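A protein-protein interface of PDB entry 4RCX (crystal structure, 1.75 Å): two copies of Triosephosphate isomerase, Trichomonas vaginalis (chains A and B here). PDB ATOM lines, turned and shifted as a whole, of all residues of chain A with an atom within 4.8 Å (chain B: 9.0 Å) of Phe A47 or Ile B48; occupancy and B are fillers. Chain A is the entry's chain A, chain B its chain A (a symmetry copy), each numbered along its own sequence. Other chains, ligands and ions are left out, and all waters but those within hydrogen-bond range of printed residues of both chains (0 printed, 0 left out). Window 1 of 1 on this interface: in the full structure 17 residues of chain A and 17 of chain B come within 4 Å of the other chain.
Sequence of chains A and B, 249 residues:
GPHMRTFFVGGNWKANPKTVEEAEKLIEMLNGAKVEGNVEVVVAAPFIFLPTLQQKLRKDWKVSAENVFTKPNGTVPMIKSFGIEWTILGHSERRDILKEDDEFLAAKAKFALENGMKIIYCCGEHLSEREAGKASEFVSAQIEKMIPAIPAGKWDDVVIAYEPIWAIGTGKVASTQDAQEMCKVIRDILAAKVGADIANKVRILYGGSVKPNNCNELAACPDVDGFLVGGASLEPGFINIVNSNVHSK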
ATOM      1  N   ALA A  45     -17.149 -23.434  23.627  1.00  0.00           N
ATOM      2  CA  ALA A  45     -16.020 -22.699  23.040  1.00  0.00           C
ATOM      3  C   ALA A  45     -16.444 -22.103  21.694  1.00  0.00           C
ATOM      4  O   ALA A  45     -17.424 -22.521  21.108  1.00  0.00           O
ATOM      5  CB  ALA A  45     -14.813 -23.645  22.871  1.00  0.00           C
ATOM      6  N   PRO A  46     -15.681 -21.119  21.191  1.00  0.00           N
ATOM      7  CA  PRO A  46     -15.923 -20.594  19.843  1.00  0.00           C
ATOM      8  C   PRO A  46     -15.973 -21.731  18.815  1.00  0.00           C
ATOM      9  O   PRO A  46     -15.237 -22.734  18.966  1.00  0.00           O
ATOM     10  CB  PRO A  46     -14.684 -19.711  19.592  1.00  0.00           C
ATOM     11  CG  PRO A  46     -14.242 -19.274  20.947  1.00  0.00           C
ATOM     12  CD  PRO A  46     -14.543 -20.469  21.864  1.00  0.00           C
ATOM     13  N   PHE A  47     -16.748 -21.573  17.761  1.00  0.00           N
ATOM     14  CA  PHE A  47     -16.833 -22.613  16.740  1.00  0.00           C
ATOM     15  C   PHE A  47     -15.489 -23.062  16.174  1.00  0.00           C
ATOM     16  O   PHE A  47     -15.312 -24.251  15.952  1.00  0.00           O
ATOM     17  CB  PHE A  47     -17.702 -22.164  15.569  1.00  0.00           C
ATOM     18  CG  PHE A  47     -19.155 -22.029  15.920  1.00  0.00           C
ATOM     19  CD1 PHE A  47     -19.927 -23.147  16.161  1.00  0.00           C
ATOM     20  CD2 PHE A  47     -19.734 -20.787  16.008  1.00  0.00           C
ATOM     21  CE1 PHE A  47     -21.254 -23.027  16.497  1.00  0.00           C
ATOM     22  CE2 PHE A  47     -21.060 -20.664  16.338  1.00  0.00           C
ATOM     23  CZ  PHE A  47     -21.814 -21.793  16.592  1.00  0.00           C
ATOM     24  N   ILE A  48     -14.568 -22.120  15.940  1.00  0.00           N
ATOM     25  CA  ILE A  48     -13.306 -22.492  15.287  1.00  0.00           C
ATOM     26  C   ILE A  48     -12.442 -23.386  16.187  1.00  0.00           C
ATOM     27  O   ILE A  48     -11.590 -24.142  15.696  1.00  0.00           O
ATOM     28  CB  ILE A  48     -12.559 -21.242  14.864  1.00  0.00           C
ATOM     29  CG1 ILE A  48     -11.543 -21.590  13.784  1.00  0.00           C
ATOM     30  CG2 ILE A  48     -12.017 -20.523  16.087  1.00  0.00           C
ATOM     31  CD1 ILE A  48     -10.994 -20.343  13.118  1.00  0.00           C
ATOM     32  N   PHE A  49     -12.719 -23.374  17.489  1.00  0.00           N
ATOM     33  CA  PHE A  49     -11.995 -24.186  18.462  1.00  0.00           C
ATOM     34  C   PHE A  49     -12.718 -25.477  18.840  1.00  0.00           C
ATOM     35  O   PHE A  49     -12.139 -26.324  19.533  1.00  0.00           O
ATOM     36  CB  PHE A  49     -11.734 -23.427  19.762  1.00  0.00           C
ATOM     37  CG  PHE A  49     -10.828 -22.249  19.627  1.00  0.00           C
ATOM     38  CD1 PHE A  49      -9.795 -22.231  18.693  1.00  0.00           C
ATOM     39  CD2 PHE A  49     -10.992 -21.176  20.458  1.00  0.00           C
ATOM     40  CE1 PHE A  49      -8.951 -21.115  18.591  1.00  0.00           C
ATOM     41  CE2 PHE A  49     -10.176 -20.066  20.356  1.00  0.00           C
ATOM     42  CZ  PHE A  49      -9.153 -20.037  19.434  1.00  0.00           C
ATOM     43  N   LEU A  50     -13.964 -25.659  18.411  1.00  0.00           N
ATOM     44  CA  LEU A  50     -14.670 -26.910  18.764  1.00  0.00           C
ATOM     45  C   LEU A  50     -13.947 -28.178  18.303  1.00  0.00           C
ATOM     46  O   LEU A  50     -13.925 -29.154  19.052  1.00  0.00           O
ATOM     47  CB  LEU A  50     -16.101 -26.922  18.225  1.00  0.00           C
ATOM     48  CG  LEU A  50     -17.020 -25.894  18.919  1.00  0.00           C
ATOM     49  CD1 LEU A  50     -18.423 -25.857  18.325  1.00  0.00           C
ATOM     50  CD2 LEU A  50     -17.039 -26.044  20.437  1.00  0.00           C
ATOM     51  N   PRO A  51     -13.384 -28.209  17.081  1.00  0.00           N
ATOM     52  CA  PRO A  51     -12.785 -29.505  16.738  1.00  0.00           C
ATOM     53  C   PRO A  51     -11.580 -29.832  17.637  1.00  0.00           C
ATOM     54  O   PRO A  51     -11.345 -31.002  17.967  1.00  0.00           O
ATOM     55  CB  PRO A  51     -12.361 -29.328  15.270  1.00  0.00           C
ATOM     56  CG  PRO A  51     -13.262 -28.194  14.729  1.00  0.00           C
ATOM     57  CD  PRO A  51     -13.477 -27.293  15.918  1.00  0.00           C
ATOM     58  N   ALA A  65     -21.448 -26.195  21.825  1.00  0.00           N
ATOM     59  CA  ALA A  65     -21.454 -25.000  21.029  1.00  0.00           C
ATOM     60  C   ALA A  65     -21.965 -23.827  21.887  1.00  0.00           C
ATOM     61  O   ALA A  65     -22.691 -24.036  22.876  1.00  0.00           O
ATOM     62  CB  ALA A  65     -22.321 -25.193  19.803  1.00  0.00           C
ATOM     63  N   ASN A  67     -23.788 -21.458  20.644  1.00  0.00           N
ATOM     64  CA  ASN A  67     -25.010 -21.043  19.960  1.00  0.00           C
ATOM     65  C   ASN A  67     -25.177 -21.958  18.744  1.00  0.00           C
ATOM     66  O   ASN A  67     -24.229 -22.605  18.320  1.00  0.00           O
ATOM     67  CB  ASN A  67     -24.964 -19.575  19.516  1.00  0.00           C
ATOM     68  CG  ASN A  67     -26.266 -19.114  18.884  1.00  0.00           C
ATOM     69  OD1 ASN A  67     -27.359 -19.531  19.294  1.00  0.00           O
ATOM     70  ND2 ASN A  67     -26.161 -18.252  17.869  1.00  0.00           N
ATOM     71  N   MET A  78     -23.589 -29.913  11.368  1.00  0.00           N
ATOM     72  CA  MET A  78     -22.138 -29.736  11.336  1.00  0.00           C
ATOM     73  C   MET A  78     -21.558 -30.048  12.688  1.00  0.00           C
ATOM     74  O   MET A  78     -20.565 -30.741  12.805  1.00  0.00           O
ATOM     75  CB  MET A  78     -21.727 -28.297  10.967  1.00  0.00           C
ATOM     76  CG  MET A  78     -22.143 -27.880   9.629  1.00  0.00           C
ATOM     77  SD  MET A  78     -21.697 -26.121   9.480  1.00  0.00           S
ATOM     78  CE  MET A  78     -22.698 -25.728   8.017  1.00  0.00           C
ATOM     79  N   ILE A  79     -22.157 -29.467  13.718  1.00  0.00           N
ATOM     80  CA  ILE A  79     -21.667 -29.632  15.047  1.00  0.00           C
ATOM     81  C   ILE A  79     -21.774 -31.088  15.482  1.00  0.00           C
ATOM     82  O   ILE A  79     -20.857 -31.641  16.066  1.00  0.00           O
ATOM     83  CB  ILE A  79     -22.469 -28.685  15.987  1.00  0.00           C
ATOM     84  CG1 ILE A  79     -21.852 -27.296  15.927  1.00  0.00           C
ATOM     85  CG2 ILE A  79     -22.597 -29.214  17.325  1.00  0.00           C
ATOM     86  CD1 ILE A  79     -22.830 -26.200  16.314  1.00  0.00           C
ATOM     87  N   PHE A  82     -19.084 -33.596  14.362  1.00  0.00           N
ATOM     88  CA  PHE A  82     -17.889 -33.657  15.166  1.00  0.00           C
ATOM     89  C   PHE A  82     -18.136 -34.460  16.443  1.00  0.00           C
ATOM     90  O   PHE A  82     -17.199 -34.834  17.143  1.00  0.00           O
ATOM     91  CB  PHE A  82     -17.410 -32.249  15.487  1.00  0.00           C
ATOM     92  CG  PHE A  82     -16.718 -31.578  14.332  1.00  0.00           C
ATOM     93  CD1 PHE A  82     -15.364 -31.797  14.099  1.00  0.00           C
ATOM     94  CD2 PHE A  82     -17.405 -30.721  13.491  1.00  0.00           C
ATOM     95  CE1 PHE A  82     -14.726 -31.170  13.030  1.00  0.00           C
ATOM     96  CE2 PHE A  82     -16.795 -30.110  12.445  1.00  0.00           C
ATOM     97  CZ  PHE A  82     -15.442 -30.331  12.194  1.00  0.00           C
ATOM     98  N   ILE A  84     -20.356 -33.453  18.795  1.00  0.00           N
ATOM     99  CA  ILE A  84     -20.730 -32.478  19.842  1.00  0.00           C
ATOM    100  C   ILE A  84     -22.221 -32.580  20.136  1.00  0.00           C
ATOM    101  O   ILE A  84     -23.018 -32.642  19.220  1.00  0.00           O
ATOM    102  CB  ILE A  84     -20.329 -31.063  19.416  1.00  0.00           C
ATOM    103  CG1 ILE A  84     -18.801 -31.009  19.469  1.00  0.00           C
ATOM    104  CG2 ILE A  84     -21.007 -29.951  20.321  1.00  0.00           C
ATOM    105  CD1 ILE A  84     -18.255 -29.957  18.572  1.00  0.00           C
ATOM    106  N   TRP B  13     -18.813 -21.372   0.579  1.00  0.00           N
ATOM    107  CA  TRP B  13     -19.592 -22.554   0.831  1.00  0.00           C
ATOM    108  C   TRP B  13     -20.858 -22.187   1.569  1.00  0.00           C
ATOM    109  O   TRP B  13     -21.758 -22.998   1.604  1.00  0.00           O
ATOM    110  CB  TRP B  13     -18.811 -23.557   1.638  1.00  0.00           C
ATOM    111  CG  TRP B  13     -17.663 -24.175   0.931  1.00  0.00           C
ATOM    112  CD1 TRP B  13     -17.194 -23.929  -0.344  1.00  0.00           C
ATOM    113  CD2 TRP B  13     -16.840 -25.205   1.478  1.00  0.00           C
ATOM    114  NE1 TRP B  13     -16.101 -24.747  -0.592  1.00  0.00           N
ATOM    115  CE2 TRP B  13     -15.877 -25.538   0.515  1.00  0.00           C
ATOM    116  CE3 TRP B  13     -16.828 -25.869   2.715  1.00  0.00           C
ATOM    117  CZ2 TRP B  13     -14.886 -26.501   0.759  1.00  0.00           C
ATOM    118  CZ3 TRP B  13     -15.871 -26.834   2.937  1.00  0.00           C
ATOM    119  CH2 TRP B  13     -14.926 -27.155   1.950  1.00  0.00           C
ATOM    120  N   LYS B  14     -20.928 -20.971   2.128  1.00  0.00           N
ATOM    121  CA  LYS B  14     -22.059 -20.544   2.984  1.00  0.00           C
ATOM    122  C   LYS B  14     -22.246 -21.538   4.128  1.00  0.00           C
ATOM    123  O   LYS B  14     -21.247 -22.003   4.641  1.00  0.00           O
ATOM    124  CB  LYS B  14     -23.317 -20.369   2.159  1.00  0.00           C
ATOM    125  CG  LYS B  14     -23.098 -19.310   1.063  1.00  0.00           C
ATOM    126  CD  LYS B  14     -24.337 -19.261   0.154  1.00  0.00           C
ATOM    127  CE  LYS B  14     -24.137 -18.215  -0.914  1.00  0.00           C
ATOM    128  NZ  LYS B  14     -25.466 -17.773  -1.428  1.00  0.00           N
ATOM    129  N   ALA B  15     -23.460 -21.895   4.522  1.00  0.00           N
ATOM    130  CA  ALA B  15     -23.584 -22.897   5.617  1.00  0.00           C
ATOM    131  C   ALA B  15     -23.680 -24.350   5.065  1.00  0.00           C
ATOM    132  O   ALA B  15     -24.689 -25.034   5.221  1.00  0.00           O
ATOM    133  CB  ALA B  15     -24.751 -22.587   6.504  1.00  0.00           C
ATOM    134  N   ASN B  16     -22.587 -24.789   4.444  1.00  0.00           N
ATOM    135  CA  ASN B  16     -22.493 -26.095   3.808  1.00  0.00           C
ATOM    136  C   ASN B  16     -21.025 -26.539   3.880  1.00  0.00           C
ATOM    137  O   ASN B  16     -20.129 -25.735   4.143  1.00  0.00           O
ATOM    138  CB  ASN B  16     -22.931 -26.044   2.347  1.00  0.00           C
ATOM    139  CG  ASN B  16     -24.314 -25.457   2.154  1.00  0.00           C
ATOM    140  OD1 ASN B  16     -24.489 -24.252   1.904  1.00  0.00           O
ATOM    141  ND2 ASN B  16     -25.295 -26.310   2.223  1.00  0.00           N
ATOM    142  N   PRO B  17     -20.774 -27.842   3.700  1.00  0.00           N
ATOM    143  CA  PRO B  17     -21.759 -28.916   3.656  1.00  0.00           C
ATOM    144  C   PRO B  17     -22.218 -29.219   5.071  1.00  0.00           C
ATOM    145  O   PRO B  17     -21.813 -28.510   5.992  1.00  0.00           O
ATOM    146  CB  PRO B  17     -20.983 -30.075   3.077  1.00  0.00           C
ATOM    147  CG  PRO B  17     -19.596 -29.832   3.563  1.00  0.00           C
ATOM    148  CD  PRO B  17     -19.394 -28.345   3.562  1.00  0.00           C
ATOM    149  N   LYS B  18     -23.042 -30.248   5.242  1.00  0.00           N
ATOM    150  CA  LYS B  18     -23.672 -30.480   6.554  1.00  0.00           C
ATOM    151  C   LYS B  18     -22.722 -31.231   7.489  1.00  0.00           C
ATOM    152  O   LYS B  18     -22.941 -31.235   8.703  1.00  0.00           O
ATOM    153  CB  LYS B  18     -25.019 -31.229   6.395  1.00  0.00           C
ATOM    154  N   THR B  19     -21.667 -31.862   6.949  1.00  0.00           N
ATOM    155  CA  THR B  19     -20.802 -32.671   7.794  1.00  0.00           C
ATOM    156  C   THR B  19     -19.328 -32.591   7.450  1.00  0.00           C
ATOM    157  O   THR B  19     -18.943 -32.371   6.304  1.00  0.00           O
ATOM    158  CB  THR B  19     -21.179 -34.163   7.741  1.00  0.00           C
ATOM    159  OG1 THR B  19     -20.840 -34.704   6.454  1.00  0.00           O
ATOM    160  CG2 THR B  19     -22.651 -34.368   8.033  1.00  0.00           C
ATOM    161  N   VAL B  20     -18.490 -32.813   8.458  1.00  0.00           N
ATOM    162  CA  VAL B  20     -17.047 -32.765   8.221  1.00  0.00           C
ATOM    163  C   VAL B  20     -16.613 -33.845   7.200  1.00  0.00           C
ATOM    164  O   VAL B  20     -15.703 -33.606   6.417  1.00  0.00           O
ATOM    165  CB  VAL B  20     -16.277 -32.875   9.551  1.00  0.00           C
ATOM    166  CG1 VAL B  20     -16.530 -34.183  10.186  1.00  0.00           C
ATOM    167  CG2 VAL B  20     -14.772 -32.632   9.349  1.00  0.00           C
ATOM    168  N   ALA B  23     -17.178 -32.335   3.835  1.00  0.00           N
ATOM    169  CA  ALA B  23     -16.217 -31.247   3.583  1.00  0.00           C
ATOM    170  C   ALA B  23     -14.911 -31.870   3.132  1.00  0.00           C
ATOM    171  O   ALA B  23     -14.265 -31.388   2.227  1.00  0.00           O
ATOM    172  CB  ALA B  23     -15.984 -30.376   4.846  1.00  0.00           C
ATOM    173  N   ALA B  45     -15.458 -20.917   4.207  1.00  0.00           N
ATOM    174  CA  ALA B  45     -16.200 -22.051   4.777  1.00  0.00           C
ATOM    175  C   ALA B  45     -16.721 -21.672   6.167  1.00  0.00           C
ATOM    176  O   ALA B  45     -16.248 -20.733   6.776  1.00  0.00           O
ATOM    177  CB  ALA B  45     -15.284 -23.290   4.847  1.00  0.00           C
ATOM    178  N   PRO B  46     -17.704 -22.430   6.680  1.00  0.00           N
ATOM    179  CA  PRO B  46     -18.160 -22.236   8.060  1.00  0.00           C
ATOM    180  C   PRO B  46     -16.978 -22.266   9.035  1.00  0.00           C
ATOM    181  O   PRO B  46     -16.005 -23.022   8.805  1.00  0.00           O
ATOM    182  CB  PRO B  46     -19.069 -23.460   8.296  1.00  0.00           C
ATOM    183  CG  PRO B  46     -19.579 -23.827   6.944  1.00  0.00           C
ATOM    184  CD  PRO B  46     -18.418 -23.517   5.987  1.00  0.00           C
ATOM    185  N   PHE B  47     -17.064 -21.537  10.129  1.00  0.00           N
ATOM    186  CA  PHE B  47     -15.977 -21.528  11.104  1.00  0.00           C
ATOM    187  C   PHE B  47     -15.544 -22.909  11.587  1.00  0.00           C
ATOM    188  O   PHE B  47     -14.352 -23.129  11.746  1.00  0.00           O
ATOM    189  CB  PHE B  47     -16.347 -20.702  12.332  1.00  0.00           C
ATOM    190  CG  PHE B  47     -16.453 -19.231  12.054  1.00  0.00           C
ATOM    191  CD1 PHE B  47     -15.325 -18.481  11.797  1.00  0.00           C
ATOM    192  CD2 PHE B  47     -17.681 -18.614  12.050  1.00  0.00           C
ATOM    193  CE1 PHE B  47     -15.420 -17.136  11.527  1.00  0.00           C
ATOM    194  CE2 PHE B  47     -17.778 -17.271  11.786  1.00  0.00           C
ATOM    195  CZ  PHE B  47     -16.640 -16.538  11.514  1.00  0.00           C
ATOM    196  N   ILE B  48     -16.502 -23.812  11.823  1.00  0.00           N
ATOM    197  CA  ILE B  48     -16.139 -25.113  12.401  1.00  0.00           C
ATOM    198  C   ILE B  48     -15.313 -25.960  11.422  1.00  0.00           C
ATOM    199  O   ILE B  48     -14.562 -26.855  11.839  1.00  0.00           O
ATOM    200  CB  ILE B  48     -17.391 -25.844  12.847  1.00  0.00           C
ATOM    201  CG1 ILE B  48     -17.026 -26.919  13.863  1.00  0.00           C
ATOM    202  CG2 ILE B  48     -18.181 -26.309  11.635  1.00  0.00           C
ATOM    203  CD1 ILE B  48     -18.257 -27.462  14.561  1.00  0.00           C
ATOM    204  N   PHE B  49     -15.375 -25.622  10.136  1.00  0.00           N
ATOM    205  CA  PHE B  49     -14.631 -26.324   9.095  1.00  0.00           C
ATOM    206  C   PHE B  49     -13.336 -25.620   8.691  1.00  0.00           C
ATOM    207  O   PHE B  49     -12.540 -26.190   7.934  1.00  0.00           O
ATOM    208  CB  PHE B  49     -15.454 -26.503   7.821  1.00  0.00           C
ATOM    209  CG  PHE B  49     -16.653 -27.380   7.969  1.00  0.00           C
ATOM    210  CD1 PHE B  49     -16.659 -28.454   8.856  1.00  0.00           C
ATOM    211  CD2 PHE B  49     -17.756 -27.148   7.197  1.00  0.00           C
ATOM    212  CE1 PHE B  49     -17.794 -29.271   8.972  1.00  0.00           C
ATOM    213  CE2 PHE B  49     -18.884 -27.936   7.314  1.00  0.00           C
ATOM    214  CZ  PHE B  49     -18.902 -28.999   8.189  1.00  0.00           C
ATOM    215  N   LEU B  50     -13.097 -24.401   9.166  1.00  0.00           N
ATOM    216  CA  LEU B  50     -11.843 -23.715   8.788  1.00  0.00           C
ATOM    217  C   LEU B  50     -10.578 -24.494   9.157  1.00  0.00           C
ATOM    218  O   LEU B  50      -9.638 -24.509   8.363  1.00  0.00           O
ATOM    219  CB  LEU B  50     -11.764 -22.311   9.390  1.00  0.00           C
ATOM    220  CG  LEU B  50     -12.794 -21.333   8.785  1.00  0.00           C
ATOM    221  CD1 LEU B  50     -12.762 -19.958   9.443  1.00  0.00           C
ATOM    222  CD2 LEU B  50     -12.711 -21.247   7.265  1.00  0.00           C
ATOM    223  N   PRO B  51     -10.509 -25.114  10.349  1.00  0.00           N
ATOM    224  CA  PRO B  51      -9.218 -25.764  10.604  1.00  0.00           C
ATOM    225  C   PRO B  51      -8.968 -26.935   9.638  1.00  0.00           C
ATOM    226  O   PRO B  51      -7.821 -27.187   9.244  1.00  0.00           O
ATOM    227  CB  PRO B  51      -9.341 -26.250  12.059  1.00  0.00           C
ATOM    228  CG  PRO B  51     -10.422 -25.344  12.691  1.00  0.00           C
ATOM    229  CD  PRO B  51     -11.369 -25.049  11.556  1.00  0.00           C
ATOM    230  N   THR B  52     -10.031 -27.659   9.295  1.00  0.00           N
ATOM    231  CA  THR B  52      -9.945 -28.728   8.307  1.00  0.00           C
ATOM    232  C   THR B  52      -9.492 -28.213   6.928  1.00  0.00           C
ATOM    233  O   THR B  52      -8.552 -28.755   6.341  1.00  0.00           O
ATOM    234  CB  THR B  52     -11.301 -29.409   8.162  1.00  0.00           C
ATOM    235  OG1 THR B  52     -11.558 -30.137   9.360  1.00  0.00           O
ATOM    236  CG2 THR B  52     -11.318 -30.356   6.960  1.00  0.00           C
ATOM    237  N   LEU B  53     -10.137 -27.162   6.438  1.00  0.00           N
ATOM    238  CA  LEU B  53      -9.724 -26.527   5.177  1.00  0.00           C
ATOM    239  C   LEU B  53      -8.263 -26.107   5.230  1.00  0.00           C
ATOM    240  O   LEU B  53      -7.453 -26.329   4.308  1.00  0.00           O
ATOM    241  CB  LEU B  53     -10.618 -25.325   4.900  1.00  0.00           C
ATOM    242  CG  LEU B  53     -10.949 -24.971   3.477  1.00  0.00           C
ATOM    243  CD1 LEU B  53     -11.388 -26.170   2.746  1.00  0.00           C
ATOM    244  CD2 LEU B  53     -12.048 -23.881   3.445  1.00  0.00           C
ATOM    245  N   GLN B  54      -7.902 -25.486   6.327  1.00  0.00           N
ATOM    246  CA  GLN B  54      -6.569 -24.906   6.406  1.00  0.00           C
ATOM    247  C   GLN B  54      -5.506 -26.022   6.388  1.00  0.00           C
ATOM    248  O   GLN B  54      -4.474 -25.900   5.693  1.00  0.00           O
ATOM    249  CB  GLN B  54      -6.467 -24.021   7.656  1.00  0.00           C
ATOM    250  CG  GLN B  54      -5.136 -23.327   7.850  1.00  0.00           C
ATOM    251  CD  GLN B  54      -4.754 -22.388   6.705  1.00  0.00           C
ATOM    252  OE1 GLN B  54      -5.606 -21.828   5.988  1.00  0.00           O
ATOM    253  NE2 GLN B  54      -3.436 -22.209   6.525  1.00  0.00           N
ATOM    254  N   GLU B  66     -16.071 -16.551   6.558  1.00  0.00           N
ATOM    255  CA  GLU B  66     -17.234 -16.041   5.830  1.00  0.00           C
ATOM    256  C   GLU B  66     -17.683 -14.711   6.428  1.00  0.00           C
ATOM    257  O   GLU B  66     -18.528 -14.009   5.863  1.00  0.00           O
ATOM    258  CB  GLU B  66     -18.384 -17.081   5.880  1.00  0.00           C
ATOM    259  CG  GLU B  66     -18.098 -18.368   5.093  1.00  0.00           C
ATOM    260  CD  GLU B  66     -19.227 -19.389   5.127  1.00  0.00           C
ATOM    261  OE1 GLU B  66     -20.241 -19.166   5.811  1.00  0.00           O
ATOM    262  OE2 GLU B  66     -19.073 -20.463   4.506  1.00  0.00           O
ATOM    263  N   THR B  75     -13.517 -13.983  16.020  1.00  0.00           N
ATOM    264  CA  THR B  75     -12.670 -12.810  15.964  1.00  0.00           C
ATOM    265  C   THR B  75     -11.385 -13.020  15.122  1.00  0.00           C
ATOM    266  O   THR B  75     -10.942 -14.143  14.818  1.00  0.00           O
ATOM    267  CB  THR B  75     -12.258 -12.333  17.376  1.00  0.00           C
ATOM    268  OG1 THR B  75     -11.276 -13.223  17.928  1.00  0.00           O
ATOM    269  CG2 THR B  75     -13.443 -12.237  18.298  1.00  0.00           C
ATOM    270  N   MET B  78      -8.242 -15.236  16.430  1.00  0.00           N
ATOM    271  CA  MET B  78      -8.461 -16.682  16.406  1.00  0.00           C
ATOM    272  C   MET B  78      -8.228 -17.207  15.016  1.00  0.00           C
ATOM    273  O   MET B  78      -7.571 -18.212  14.822  1.00  0.00           O
ATOM    274  CB  MET B  78      -9.894 -17.069  16.822  1.00  0.00           C
ATOM    275  CG  MET B  78     -10.237 -16.704  18.195  1.00  0.00           C
ATOM    276  SD  MET B  78     -12.001 -17.107  18.405  1.00  0.00           S
ATOM    277  CE  MET B  78     -12.298 -16.164  19.928  1.00  0.00           C
ATOM    278  N   ILE B  79      -8.837 -16.544  14.041  1.00  0.00           N
ATOM    279  CA  ILE B  79      -8.746 -16.977  12.685  1.00  0.00           C
ATOM    280  C   ILE B  79      -7.309 -16.891  12.189  1.00  0.00           C
ATOM    281  O   ILE B  79      -6.811 -17.795  11.539  1.00  0.00           O
ATOM    282  CB  ILE B  79      -9.710 -16.106  11.827  1.00  0.00           C
ATOM    283  CG1 ILE B  79     -11.113 -16.686  11.924  1.00  0.00           C
ATOM    284  CG2 ILE B  79      -9.238 -15.931  10.473  1.00  0.00           C
ATOM    285  CD1 ILE B  79     -12.196 -15.660  11.633  1.00  0.00           C
ATOM    286  N   PHE B  82      -4.836 -19.700  13.069  1.00  0.00           N
ATOM    287  CA  PHE B  82      -4.847 -20.857  12.210  1.00  0.00           C
ATOM    288  C   PHE B  82      -4.095 -20.574  10.910  1.00  0.00           C
ATOM    289  O   PHE B  82      -3.782 -21.487  10.152  1.00  0.00           O
ATOM    290  CB  PHE B  82      -6.282 -21.280  11.933  1.00  0.00           C
ATOM    291  CG  PHE B  82      -6.921 -22.006  13.087  1.00  0.00           C
ATOM    292  CD1 PHE B  82      -6.732 -23.375  13.248  1.00  0.00           C
ATOM    293  CD2 PHE B  82      -7.718 -21.336  13.996  1.00  0.00           C
ATOM    294  CE1 PHE B  82      -7.330 -24.044  14.315  1.00  0.00           C
ATOM    295  CE2 PHE B  82      -8.300 -21.976  15.041  1.00  0.00           C
ATOM    296  CZ  PHE B  82      -8.108 -23.345  15.221  1.00  0.00           C
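Pro A46 touches Met B78, and with the chains exchanged Met A78 touches Pro B46.
Phe A47 touches Ile B48, and with the chains exchanged Ile A48 touches Phe B47.
Phe A49 touches Met B78, and with the chains exchanged Met A78 touches Phe B49.
Phe A49 touches Phe B82, and with the chains exchanged Phe A82 touches Phe B49.
Of the 20 pairs that touch across the chains among the printed residues, 15 have their exchanged pair printed and touching as well.
O of Ile A79 sits at hydrogen-bond distance from N of Ile A84, 3.3 Å away.
O of Trp B13 sits close to OD1 of Asn B16, at 3.0 Å.
Among the printed residues, pairs that only touch across the chains: Met A78 with Ala B15 (3.4 Å), Pro A51 with Ile B48 (3.4 Å), Ile A48 with Pro B51 (3.4 Å), Ile A48 with Phe B82 (3.5 Å), Phe A82 with Ile B48 (3.5 Å), Met A78 with Pro B17 (3.6 Å), Met A78 with Asn B16 (3.7 Å), Phe A82 with Phe B49 (3.7 Å), Phe A49 with Phe B82 (3.7 Å), Phe A49 with Met B78 (3.7 Å), Met A78 with Phe B49 (3.7 Å), Phe A82 with Val B20 (3.7 Å), Phe A47 with Ile B48 (3.7 Å), Ile A48 with Phe B47 (3.7 Å), Phe A47 with Phe B47 (3.8 Å), Pro A46 with Met B78 (3.8 Å), Met A78 with Pro B46 (3.8 Å), Ile A48 with Ile B79 (3.8 Å) and Ile A79 with Ile B48 (3.8 Å).
Hydrophobic or aromatic side chains of chain A within 4 Å of the printed part of chain B: Pro A46, Phe A47, Ile A48, Phe A49, Pro A51, Met A78, Ile A79 and Phe A82.
Of the 24 printed residues of chain B, 13 touch a printed residue of chain A.
Printed residues of chain B that touch a printed residue of chain A: Ala B15, Asn B16, Pro B17, Lys B18, Val B20, Pro B46, Phe B47, Ile B48, Phe B49, Pro B51, Met B78, Ile B79 and Phe B82.
Among the printed residues, 20 pairs touch across the chains.
Among the printed residues, no Asp or Glu carboxylate lies within 4 Å of a Lys or Arg side-chain nitrogen of the other chain.
The backbone NH (N) of Met A78 sits at hydrogen-bond distance from the backbone carbonyl oxygen (O) of Lys B18.
Of the printed residues of chain A, Ile B48 touches Phe A47 (3.7 Å), Pro A51 (3.4 Å), Ile A79 (3.8 Å) and Phe A82 (3.5 Å).
Pro A46 touches just one residue of chain B: Met B78 (3.8 Å).
Of the printed residues of chain A, Asn B16 touches Met A78.
Of the printed residues of chain B, Phe A49 touches Met B78 (3.7 Å) and Phe B82 (3.7 Å).
Printed residues of chain B within 4 Å of Pro A51: Ile B48 (3.4 Å).
Of the printed residues of chain B, Met A78 touches Ala B15 (3.4 Å), Asn B16 (3.7 Å), Pro B17 (3.6 Å), Lys B18 (3.0 Å), Pro B46 (3.8 Å) and Phe B49 (3.7 Å).
The nearest printed residue of chain B that does not touch Phe A47 is Pro B51 (6.0 Å).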
